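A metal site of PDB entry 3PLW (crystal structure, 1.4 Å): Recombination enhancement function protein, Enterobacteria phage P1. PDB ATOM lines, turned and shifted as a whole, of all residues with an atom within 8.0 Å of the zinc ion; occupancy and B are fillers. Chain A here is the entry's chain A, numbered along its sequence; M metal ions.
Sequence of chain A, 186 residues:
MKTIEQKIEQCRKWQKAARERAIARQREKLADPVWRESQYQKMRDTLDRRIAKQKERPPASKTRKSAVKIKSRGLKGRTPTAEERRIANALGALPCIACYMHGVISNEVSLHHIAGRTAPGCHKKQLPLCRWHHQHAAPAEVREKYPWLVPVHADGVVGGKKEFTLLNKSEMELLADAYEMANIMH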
ATOM      1  N   PRO A  95      18.292  21.037  -5.006  1.00  0.00           N
ATOM      2  CA  PRO A  95      17.462  22.225  -5.278  1.00  0.00           C
ATOM      3  C   PRO A  95      16.730  22.074  -6.620  1.00  0.00           C
ATOM      4  O   PRO A  95      16.953  21.096  -7.355  1.00  0.00           O
ATOM      5  CB  PRO A  95      18.490  23.350  -5.351  1.00  0.00           C
ATOM      6  CG  PRO A  95      19.700  22.680  -5.929  1.00  0.00           C
ATOM      7  CD  PRO A  95      19.709  21.280  -5.321  1.00  0.00           C
ATOM      8  N   CYS A  96      15.861  23.035  -6.937  1.00  0.00           N
ATOM      9  CA  CYS A  96      15.042  22.933  -8.147  1.00  0.00           C
ATOM     10  C   CYS A  96      15.940  22.809  -9.371  1.00  0.00           C
ATOM     11  O   CYS A  96      16.772  23.663  -9.632  1.00  0.00           O
ATOM     12  CB  CYS A  96      14.145  24.159  -8.268  1.00  0.00           C
ATOM     13  SG  CYS A  96      13.196  24.165  -9.802  1.00  0.00           S
ATOM     14  N   ILE A  97      15.760  21.750 -10.155  1.00  0.00           N
ATOM     15  CA  ILE A  97      16.658  21.504 -11.258  1.00  0.00           C
ATOM     16  C   ILE A  97      16.390  22.440 -12.444  1.00  0.00           C
ATOM     17  O   ILE A  97      17.300  22.710 -13.237  1.00  0.00           O
ATOM     18  CB  ILE A  97      16.601  19.999 -11.657  1.00  0.00           C
ATOM     19  CG1 ILE A  97      17.784  19.602 -12.549  1.00  0.00           C
ATOM     20  CG2 ILE A  97      15.248  19.638 -12.279  1.00  0.00           C
ATOM     21  CD1 ILE A  97      19.127  19.733 -11.885  1.00  0.00           C
ATOM     22  N   ALA A  98      15.152  22.944 -12.559  1.00  0.00           N
ATOM     23  CA  ALA A  98      14.822  23.912 -13.606  1.00  0.00           C
ATOM     24  C   ALA A  98      15.413  25.273 -13.231  1.00  0.00           C
ATOM     25  O   ALA A  98      16.061  25.909 -14.053  1.00  0.00           O
ATOM     26  CB  ALA A  98      13.324  23.984 -13.824  1.00  0.00           C
ATOM     27  N   CYS A  99      15.199  25.731 -12.004  1.00  0.00           N
ATOM     28  CA  CYS A  99      15.828  26.996 -11.556  1.00  0.00           C
ATOM     29  C   CYS A  99      17.344  26.934 -11.718  1.00  0.00           C
ATOM     30  O   CYS A  99      17.979  27.930 -12.121  1.00  0.00           O
ATOM     31  CB  CYS A  99      15.477  27.310 -10.102  1.00  0.00           C
ATOM     32  SG  CYS A  99      13.837  28.003  -9.822  1.00  0.00           S
ATOM     33  N   TYR A 100      17.934  25.772 -11.449  1.00  0.00           N
ATOM     34  CA  TYR A 100      19.377  25.619 -11.459  1.00  0.00           C
ATOM     35  C   TYR A 100      20.012  25.963 -12.813  1.00  0.00           C
ATOM     36  O   TYR A 100      21.066  26.612 -12.869  1.00  0.00           O
ATOM     37  CB  TYR A 100      19.745  24.199 -11.030  1.00  0.00           C
ATOM     38  CG  TYR A 100      21.194  24.031 -10.653  1.00  0.00           C
ATOM     39  CD1 TYR A 100      21.607  24.291  -9.350  1.00  0.00           C
ATOM     40  CD2 TYR A 100      22.134  23.607 -11.584  1.00  0.00           C
ATOM     41  CE1 TYR A 100      22.930  24.135  -8.974  1.00  0.00           C
ATOM     42  CE2 TYR A 100      23.472  23.439 -11.219  1.00  0.00           C
ATOM     43  CZ  TYR A 100      23.860  23.716  -9.914  1.00  0.00           C
ATOM     44  OH  TYR A 100      25.181  23.559  -9.547  1.00  0.00           O
ATOM     45  N   HIS A 102      19.113  28.149 -14.767  1.00  0.00           N
ATOM     46  CA  HIS A 102      19.015  29.595 -14.886  1.00  0.00           C
ATOM     47  C   HIS A 102      19.860  30.306 -13.845  1.00  0.00           C
ATOM     48  O   HIS A 102      19.778  31.524 -13.704  1.00  0.00           O
ATOM     49  CB  HIS A 102      17.546  30.000 -14.803  1.00  0.00           C
ATOM     50  CG  HIS A 102      16.758  29.531 -15.975  1.00  0.00           C
ATOM     51  ND1 HIS A 102      15.901  28.450 -15.955  1.00  0.00           N
ATOM     52  CD2 HIS A 102      16.774  29.976 -17.257  1.00  0.00           C
ATOM     53  CE1 HIS A 102      15.395  28.271 -17.169  1.00  0.00           C
ATOM     54  NE2 HIS A 102      15.899  29.190 -17.971  1.00  0.00           N
ATOM     55  N   VAL A 104      19.734  29.954 -10.601  1.00  0.00           N
ATOM     56  CA  VAL A 104      18.977  30.264  -9.375  1.00  0.00           C
ATOM     57  C   VAL A 104      18.955  29.039  -8.482  1.00  0.00           C
ATOM     58  O   VAL A 104      18.744  27.927  -8.962  1.00  0.00           O
ATOM     59  CB  VAL A 104      17.548  30.740  -9.731  1.00  0.00           C
ATOM     60  CG1 VAL A 104      16.647  30.856  -8.495  1.00  0.00           C
ATOM     61  CG2 VAL A 104      17.619  32.083 -10.479  1.00  0.00           C
ATOM     62  N   ILE A 105      19.207  29.246  -7.189  1.00  0.00           N
ATOM     63  CA  ILE A 105      19.152  28.171  -6.202  1.00  0.00           C
ATOM     64  C   ILE A 105      17.848  28.286  -5.418  1.00  0.00           C
ATOM     65  O   ILE A 105      17.661  29.196  -4.592  1.00  0.00           O
ATOM     66  CB  ILE A 105      20.375  28.172  -5.243  1.00  0.00           C
ATOM     67  CG1 ILE A 105      21.683  28.223  -6.041  1.00  0.00           C
ATOM     68  CG2 ILE A 105      20.298  26.962  -4.271  1.00  0.00           C
ATOM     69  CD1 ILE A 105      21.902  27.044  -7.003  1.00  0.00           C
ATOM     70  N   SER A 106      16.938  27.371  -5.729  1.00  0.00           N
ATOM     71  CA  SER A 106      15.613  27.321  -5.111  1.00  0.00           C
ATOM     72  C   SER A 106      15.528  26.011  -4.363  1.00  0.00           C
ATOM     73  O   SER A 106      15.284  24.972  -4.956  1.00  0.00           O
ATOM     74  CB  SER A 106      14.528  27.362  -6.188  1.00  0.00           C
ATOM     75  OG  SER A 106      14.423  28.653  -6.750  1.00  0.00           O
ATOM     76  N   ASN A 107      15.728  26.050  -3.047  1.00  0.00           N
ATOM     77  CA  ASN A 107      15.911  24.797  -2.338  1.00  0.00           C
ATOM     78  C   ASN A 107      14.693  24.233  -1.612  1.00  0.00           C
ATOM     79  O   ASN A 107      14.797  23.192  -0.959  1.00  0.00           O
ATOM     80  CB  ASN A 107      17.209  24.799  -1.493  1.00  0.00           C
ATOM     81  CG  ASN A 107      17.089  25.602  -0.241  1.00  0.00           C
ATOM     82  OD1 ASN A 107      16.041  26.173   0.074  1.00  0.00           O
ATOM     83  ND2 ASN A 107      18.190  25.669   0.508  1.00  0.00           N
ATOM     84  N   GLU A 108      13.538  24.896  -1.754  1.00  0.00           N
ATOM     85  CA  GLU A 108      12.288  24.371  -1.240  1.00  0.00           C
ATOM     86  C   GLU A 108      11.570  23.685  -2.405  1.00  0.00           C
ATOM     87  O   GLU A 108      10.965  24.351  -3.258  1.00  0.00           O
ATOM     88  CB  GLU A 108      11.443  25.469  -0.596  1.00  0.00           C
ATOM     89  CG  GLU A 108      10.297  24.970   0.276  1.00  0.00           C
ATOM     90  CD  GLU A 108      10.762  24.108   1.454  1.00  0.00           C
ATOM     91  OE1 GLU A 108      11.932  24.235   1.882  1.00  0.00           O
ATOM     92  OE2 GLU A 108       9.961  23.301   1.940  1.00  0.00           O
ATOM     93  N   VAL A 109      11.666  22.367  -2.449  1.00  0.00           N
ATOM     94  CA  VAL A 109      11.201  21.586  -3.597  1.00  0.00           C
ATOM     95  C   VAL A 109      10.262  20.458  -3.234  1.00  0.00           C
ATOM     96  O   VAL A 109      10.167  20.056  -2.065  1.00  0.00           O
ATOM     97  CB  VAL A 109      12.383  20.979  -4.389  1.00  0.00           C
ATOM     98  CG1 VAL A 109      13.342  22.083  -4.866  1.00  0.00           C
ATOM     99  CG2 VAL A 109      13.131  19.907  -3.555  1.00  0.00           C
ATOM    100  N   PRO A 128      13.234  17.266  -8.937  1.00  0.00           N
ATOM    101  CA  PRO A 128      13.011  18.207  -7.832  1.00  0.00           C
ATOM    102  C   PRO A 128      12.662  19.587  -8.403  1.00  0.00           C
ATOM    103  O   PRO A 128      13.465  20.155  -9.163  1.00  0.00           O
ATOM    104  CB  PRO A 128      14.361  18.234  -7.120  1.00  0.00           C
ATOM    105  CG  PRO A 128      15.376  17.903  -8.183  1.00  0.00           C
ATOM    106  CD  PRO A 128      14.660  17.043  -9.232  1.00  0.00           C
ATOM    107  N   LEU A 129      11.487  20.078  -8.059  1.00  0.00           N
ATOM    108  CA  LEU A 129      11.017  21.349  -8.601  1.00  0.00           C
ATOM    109  C   LEU A 129      10.479  22.242  -7.512  1.00  0.00           C
ATOM    110  O   LEU A 129       9.819  21.768  -6.590  1.00  0.00           O
ATOM    111  CB  LEU A 129       9.938  21.152  -9.689  1.00  0.00           C
ATOM    112  CG  LEU A 129      10.324  20.345 -10.923  1.00  0.00           C
ATOM    113  CD1 LEU A 129       9.101  20.103 -11.800  1.00  0.00           C
ATOM    114  CD2 LEU A 129      11.426  21.070 -11.725  1.00  0.00           C
ATOM    115  N   CYS A 130      10.767  23.539  -7.631  1.00  0.00           N
ATOM    116  CA  CYS A 130      10.170  24.533  -6.724  1.00  0.00           C
ATOM    117  C   CYS A 130       8.664  24.653  -6.976  1.00  0.00           C
ATOM    118  O   CYS A 130       8.144  24.123  -7.973  1.00  0.00           O
ATOM    119  CB  CYS A 130      10.836  25.908  -6.891  1.00  0.00           C
ATOM    120  SG  CYS A 130      10.452  26.736  -8.466  1.00  0.00           S
ATOM    121  N   ARG A 131       7.952  25.364  -6.107  1.00  0.00           N
ATOM    122  CA  ARG A 131       6.497  25.414  -6.229  1.00  0.00           C
ATOM    123  C   ARG A 131       6.048  26.040  -7.562  1.00  0.00           C
ATOM    124  O   ARG A 131       5.023  25.652  -8.133  1.00  0.00           O
ATOM    125  CB  ARG A 131       5.873  26.187  -5.054  1.00  0.00           C
ATOM    126  CG  ARG A 131       6.192  27.685  -5.033  1.00  0.00           C
ATOM    127  CD  ARG A 131       5.924  28.287  -3.637  1.00  0.00           C
ATOM    128  NE  ARG A 131       4.584  28.019  -3.120  1.00  0.00           N
ATOM    129  CZ  ARG A 131       3.503  28.739  -3.402  1.00  0.00           C
ATOM    130  NH1 ARG A 131       2.322  28.417  -2.865  1.00  0.00           N
ATOM    131  NH2 ARG A 131       3.594  29.787  -4.219  1.00  0.00           N
ATOM    132  N   TRP A 132       6.844  26.982  -8.059  1.00  0.00           N
ATOM    133  CA  TRP A 132       6.503  27.730  -9.268  1.00  0.00           C
ATOM    134  C   TRP A 132       6.826  26.959 -10.535  1.00  0.00           C
ATOM    135  O   TRP A 132       6.281  27.264 -11.591  1.00  0.00           O
ATOM    136  CB  TRP A 132       7.275  29.025  -9.293  1.00  0.00           C
ATOM    137  CG  TRP A 132       7.130  29.942  -8.107  1.00  0.00           C
ATOM    138  CD1 TRP A 132       8.143  30.405  -7.317  1.00  0.00           C
ATOM    139  CD2 TRP A 132       5.930  30.572  -7.640  1.00  0.00           C
ATOM    140  NE1 TRP A 132       7.653  31.264  -6.365  1.00  0.00           N
ATOM    141  CE2 TRP A 132       6.297  31.395  -6.540  1.00  0.00           C
ATOM    142  CE3 TRP A 132       4.580  30.513  -8.023  1.00  0.00           C
ATOM    143  CZ2 TRP A 132       5.364  32.162  -5.833  1.00  0.00           C
ATOM    144  CZ3 TRP A 132       3.647  31.280  -7.306  1.00  0.00           C
ATOM    145  CH2 TRP A 132       4.047  32.101  -6.233  1.00  0.00           C
ATOM    146  N   HIS A 133       7.719  25.976 -10.434  1.00  0.00           N
ATOM    147  CA  HIS A 133       8.050  25.106 -11.552  1.00  0.00           C
ATOM    148  C   HIS A 133       7.250  23.821 -11.513  1.00  0.00           C
ATOM    149  O   HIS A 133       7.248  23.067 -12.495  1.00  0.00           O
ATOM    150  CB  HIS A 133       9.543  24.760 -11.563  1.00  0.00           C
ATOM    151  CG  HIS A 133      10.373  25.707 -12.351  1.00  0.00           C
ATOM    152  ND1 HIS A 133      11.498  26.336 -11.827  1.00  0.00           N
ATOM    153  CD2 HIS A 133      10.270  26.122 -13.641  1.00  0.00           C
ATOM    154  CE1 HIS A 133      12.037  27.096 -12.764  1.00  0.00           C
ATOM    155  NE2 HIS A 133      11.312  26.974 -13.875  1.00  0.00           N
ATOM    156  N   HIS A 134       6.549  23.558 -10.399  1.00  0.00           N
ATOM    157  CA  HIS A 134       5.759  22.335 -10.316  1.00  0.00           C
ATOM    158  C   HIS A 134       4.274  22.543 -10.610  1.00  0.00           C
ATOM    159  O   HIS A 134       3.790  22.090 -11.651  1.00  0.00           O
ATOM    160  CB  HIS A 134       5.966  21.589  -8.994  1.00  0.00           C
ATOM    161  CG  HIS A 134       5.529  20.159  -9.073  1.00  0.00           C
ATOM    162  ND1 HIS A 134       5.258  19.388  -7.955  1.00  0.00           N
ATOM    163  CD2 HIS A 134       5.271  19.365 -10.142  1.00  0.00           C
ATOM    164  CE1 HIS A 134       4.880  18.176  -8.338  1.00  0.00           C
ATOM    165  NE2 HIS A 134       4.876  18.139  -9.656  1.00  0.00           N
ATOM    166  N   TRP A 148      11.036  32.050 -17.564  1.00  0.00           N
ATOM    167  CA  TRP A 148      11.170  30.593 -17.501  1.00  0.00           C
ATOM    168  C   TRP A 148      10.514  29.971 -16.261  1.00  0.00           C
ATOM    169  O   TRP A 148      10.449  28.732 -16.144  1.00  0.00           O
ATOM    170  CB  TRP A 148      12.660  30.225 -17.510  1.00  0.00           C
ATOM    171  CG  TRP A 148      13.485  31.146 -16.647  1.00  0.00           C
ATOM    172  CD1 TRP A 148      14.170  32.267 -17.049  1.00  0.00           C
ATOM    173  CD2 TRP A 148      13.679  31.053 -15.216  1.00  0.00           C
ATOM    174  NE1 TRP A 148      14.805  32.845 -15.972  1.00  0.00           N
ATOM    175  CE2 TRP A 148      14.529  32.118 -14.837  1.00  0.00           C
ATOM    176  CE3 TRP A 148      13.256  30.152 -14.225  1.00  0.00           C
ATOM    177  CZ2 TRP A 148      14.932  32.341 -13.509  1.00  0.00           C
ATOM    178  CZ3 TRP A 148      13.661  30.346 -12.914  1.00  0.00           C
ATOM    179  CH2 TRP A 148      14.501  31.437 -12.567  1.00  0.00           C
ATOM    180  N   LEU A 149       9.991  30.807 -15.353  1.00  0.00           N
ATOM    181  CA  LEU A 149       9.405  30.336 -14.098  1.00  0.00           C
ATOM    182  C   LEU A 149       7.935  29.959 -14.333  1.00  0.00           C
ATOM    183  O   LEU A 149       7.030  30.713 -13.965  1.00  0.00           O
ATOM    184  CB  LEU A 149       9.543  31.417 -13.034  1.00  0.00           C
ATOM    185  CG  LEU A 149       9.205  30.960 -11.607  1.00  0.00           C
ATOM    186  CD1 LEU A 149      10.340  30.070 -11.075  1.00  0.00           C
ATOM    187  CD2 LEU A 149       8.979  32.171 -10.688  1.00  0.00           C
ATOM    188  N   VAL A 150       7.720  28.808 -14.961  1.00  0.00           N
ATOM    189  CA  VAL A 150       6.369  28.334 -15.288  1.00  0.00           C
ATOM    190  C   VAL A 150       6.214  26.889 -14.782  1.00  0.00           C
ATOM    191  O   VAL A 150       7.197  26.136 -14.756  1.00  0.00           O
ATOM    192  CB  VAL A 150       6.035  28.380 -16.814  1.00  0.00           C
ATOM    193  CG1 VAL A 150       6.109  29.816 -17.326  1.00  0.00           C
ATOM    194  CG2 VAL A 150       6.961  27.497 -17.642  1.00  0.00           C
ATOM    195  N   PHE A 164       6.855  24.652 -20.368  1.00  0.00           N
ATOM    196  CA  PHE A 164       7.941  24.387 -19.435  1.00  0.00           C
ATOM    197  C   PHE A 164       9.192  23.930 -20.211  1.00  0.00           C
ATOM    198  O   PHE A 164      10.296  24.390 -19.933  1.00  0.00           O
ATOM    199  CB  PHE A 164       7.469  23.326 -18.432  1.00  0.00           C
ATOM    200  CG  PHE A 164       8.546  22.821 -17.507  1.00  0.00           C
ATOM    201  CD1 PHE A 164       9.362  21.746 -17.884  1.00  0.00           C
ATOM    202  CD2 PHE A 164       8.714  23.384 -16.241  1.00  0.00           C
ATOM    203  CE1 PHE A 164      10.358  21.258 -17.028  1.00  0.00           C
ATOM    204  CE2 PHE A 164       9.697  22.908 -15.364  1.00  0.00           C
ATOM    205  CZ  PHE A 164      10.519  21.828 -15.751  1.00  0.00           C
ATOM    206  N   ASN A 168      12.838  25.849 -20.466  1.00  0.00           N
ATOM    207  CA  ASN A 168      13.826  25.156 -19.622  1.00  0.00           C
ATOM    208  C   ASN A 168      14.551  24.090 -20.452  1.00  0.00           C
ATOM    209  O   ASN A 168      15.255  24.456 -21.402  1.00  0.00           O
ATOM    210  CB  ASN A 168      13.140  24.661 -18.338  1.00  0.00           C
ATOM    211  CG  ASN A 168      12.561  25.819 -17.529  1.00  0.00           C
ATOM    212  OD1 ASN A 168      13.277  26.475 -16.778  1.00  0.00           O
ATOM    213  ND2 ASN A 168      11.282  26.096 -17.700  1.00  0.00           N
HETATM  214 ZN    ZN M   1      12.284  26.335  -9.891  1.00  0.00          ZN
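The zinc ion is bound by a ring nitrogen (ND1) of His 133 (2.1 Å), the side-chain sulfur (SG) of Cys 99 (2.3 Å), the side-chain sulfur (SG) of Cys 96 (2.4 Å) and the side-chain sulfur (SG) of Cys 130 (2.4 Å).
SG of Cys 130 lies close to N of Trp 132 (3.6 Å).
N of Cys 96 sits at hydrogen-bond distance from O of Ser 106 (2.8 Å).
The backbone carbonyl oxygen of Cys 99 lies within hydrogen-bond range of the backbone NH of Val 104, at 3.1 Å.
A ring nitrogen (NE2) of His 133 lies within hydrogen-bond range of the backbone carbonyl oxygen (O) of Trp 148 (3.0 Å).
The side-chain sulfur of Cys 96 sits close to the backbone NH of Ala 98, at 3.6 Å.
The side-chain sulfur of Cys 99 lies close to the side-chain hydroxyl of Ser 106 (3.2 Å).
Of the 25 residues printed, 4 come within 4 Å of the zinc ion.
The nearest printed residue that does not touch the zinc ion is Leu 149 (4.4 Å).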
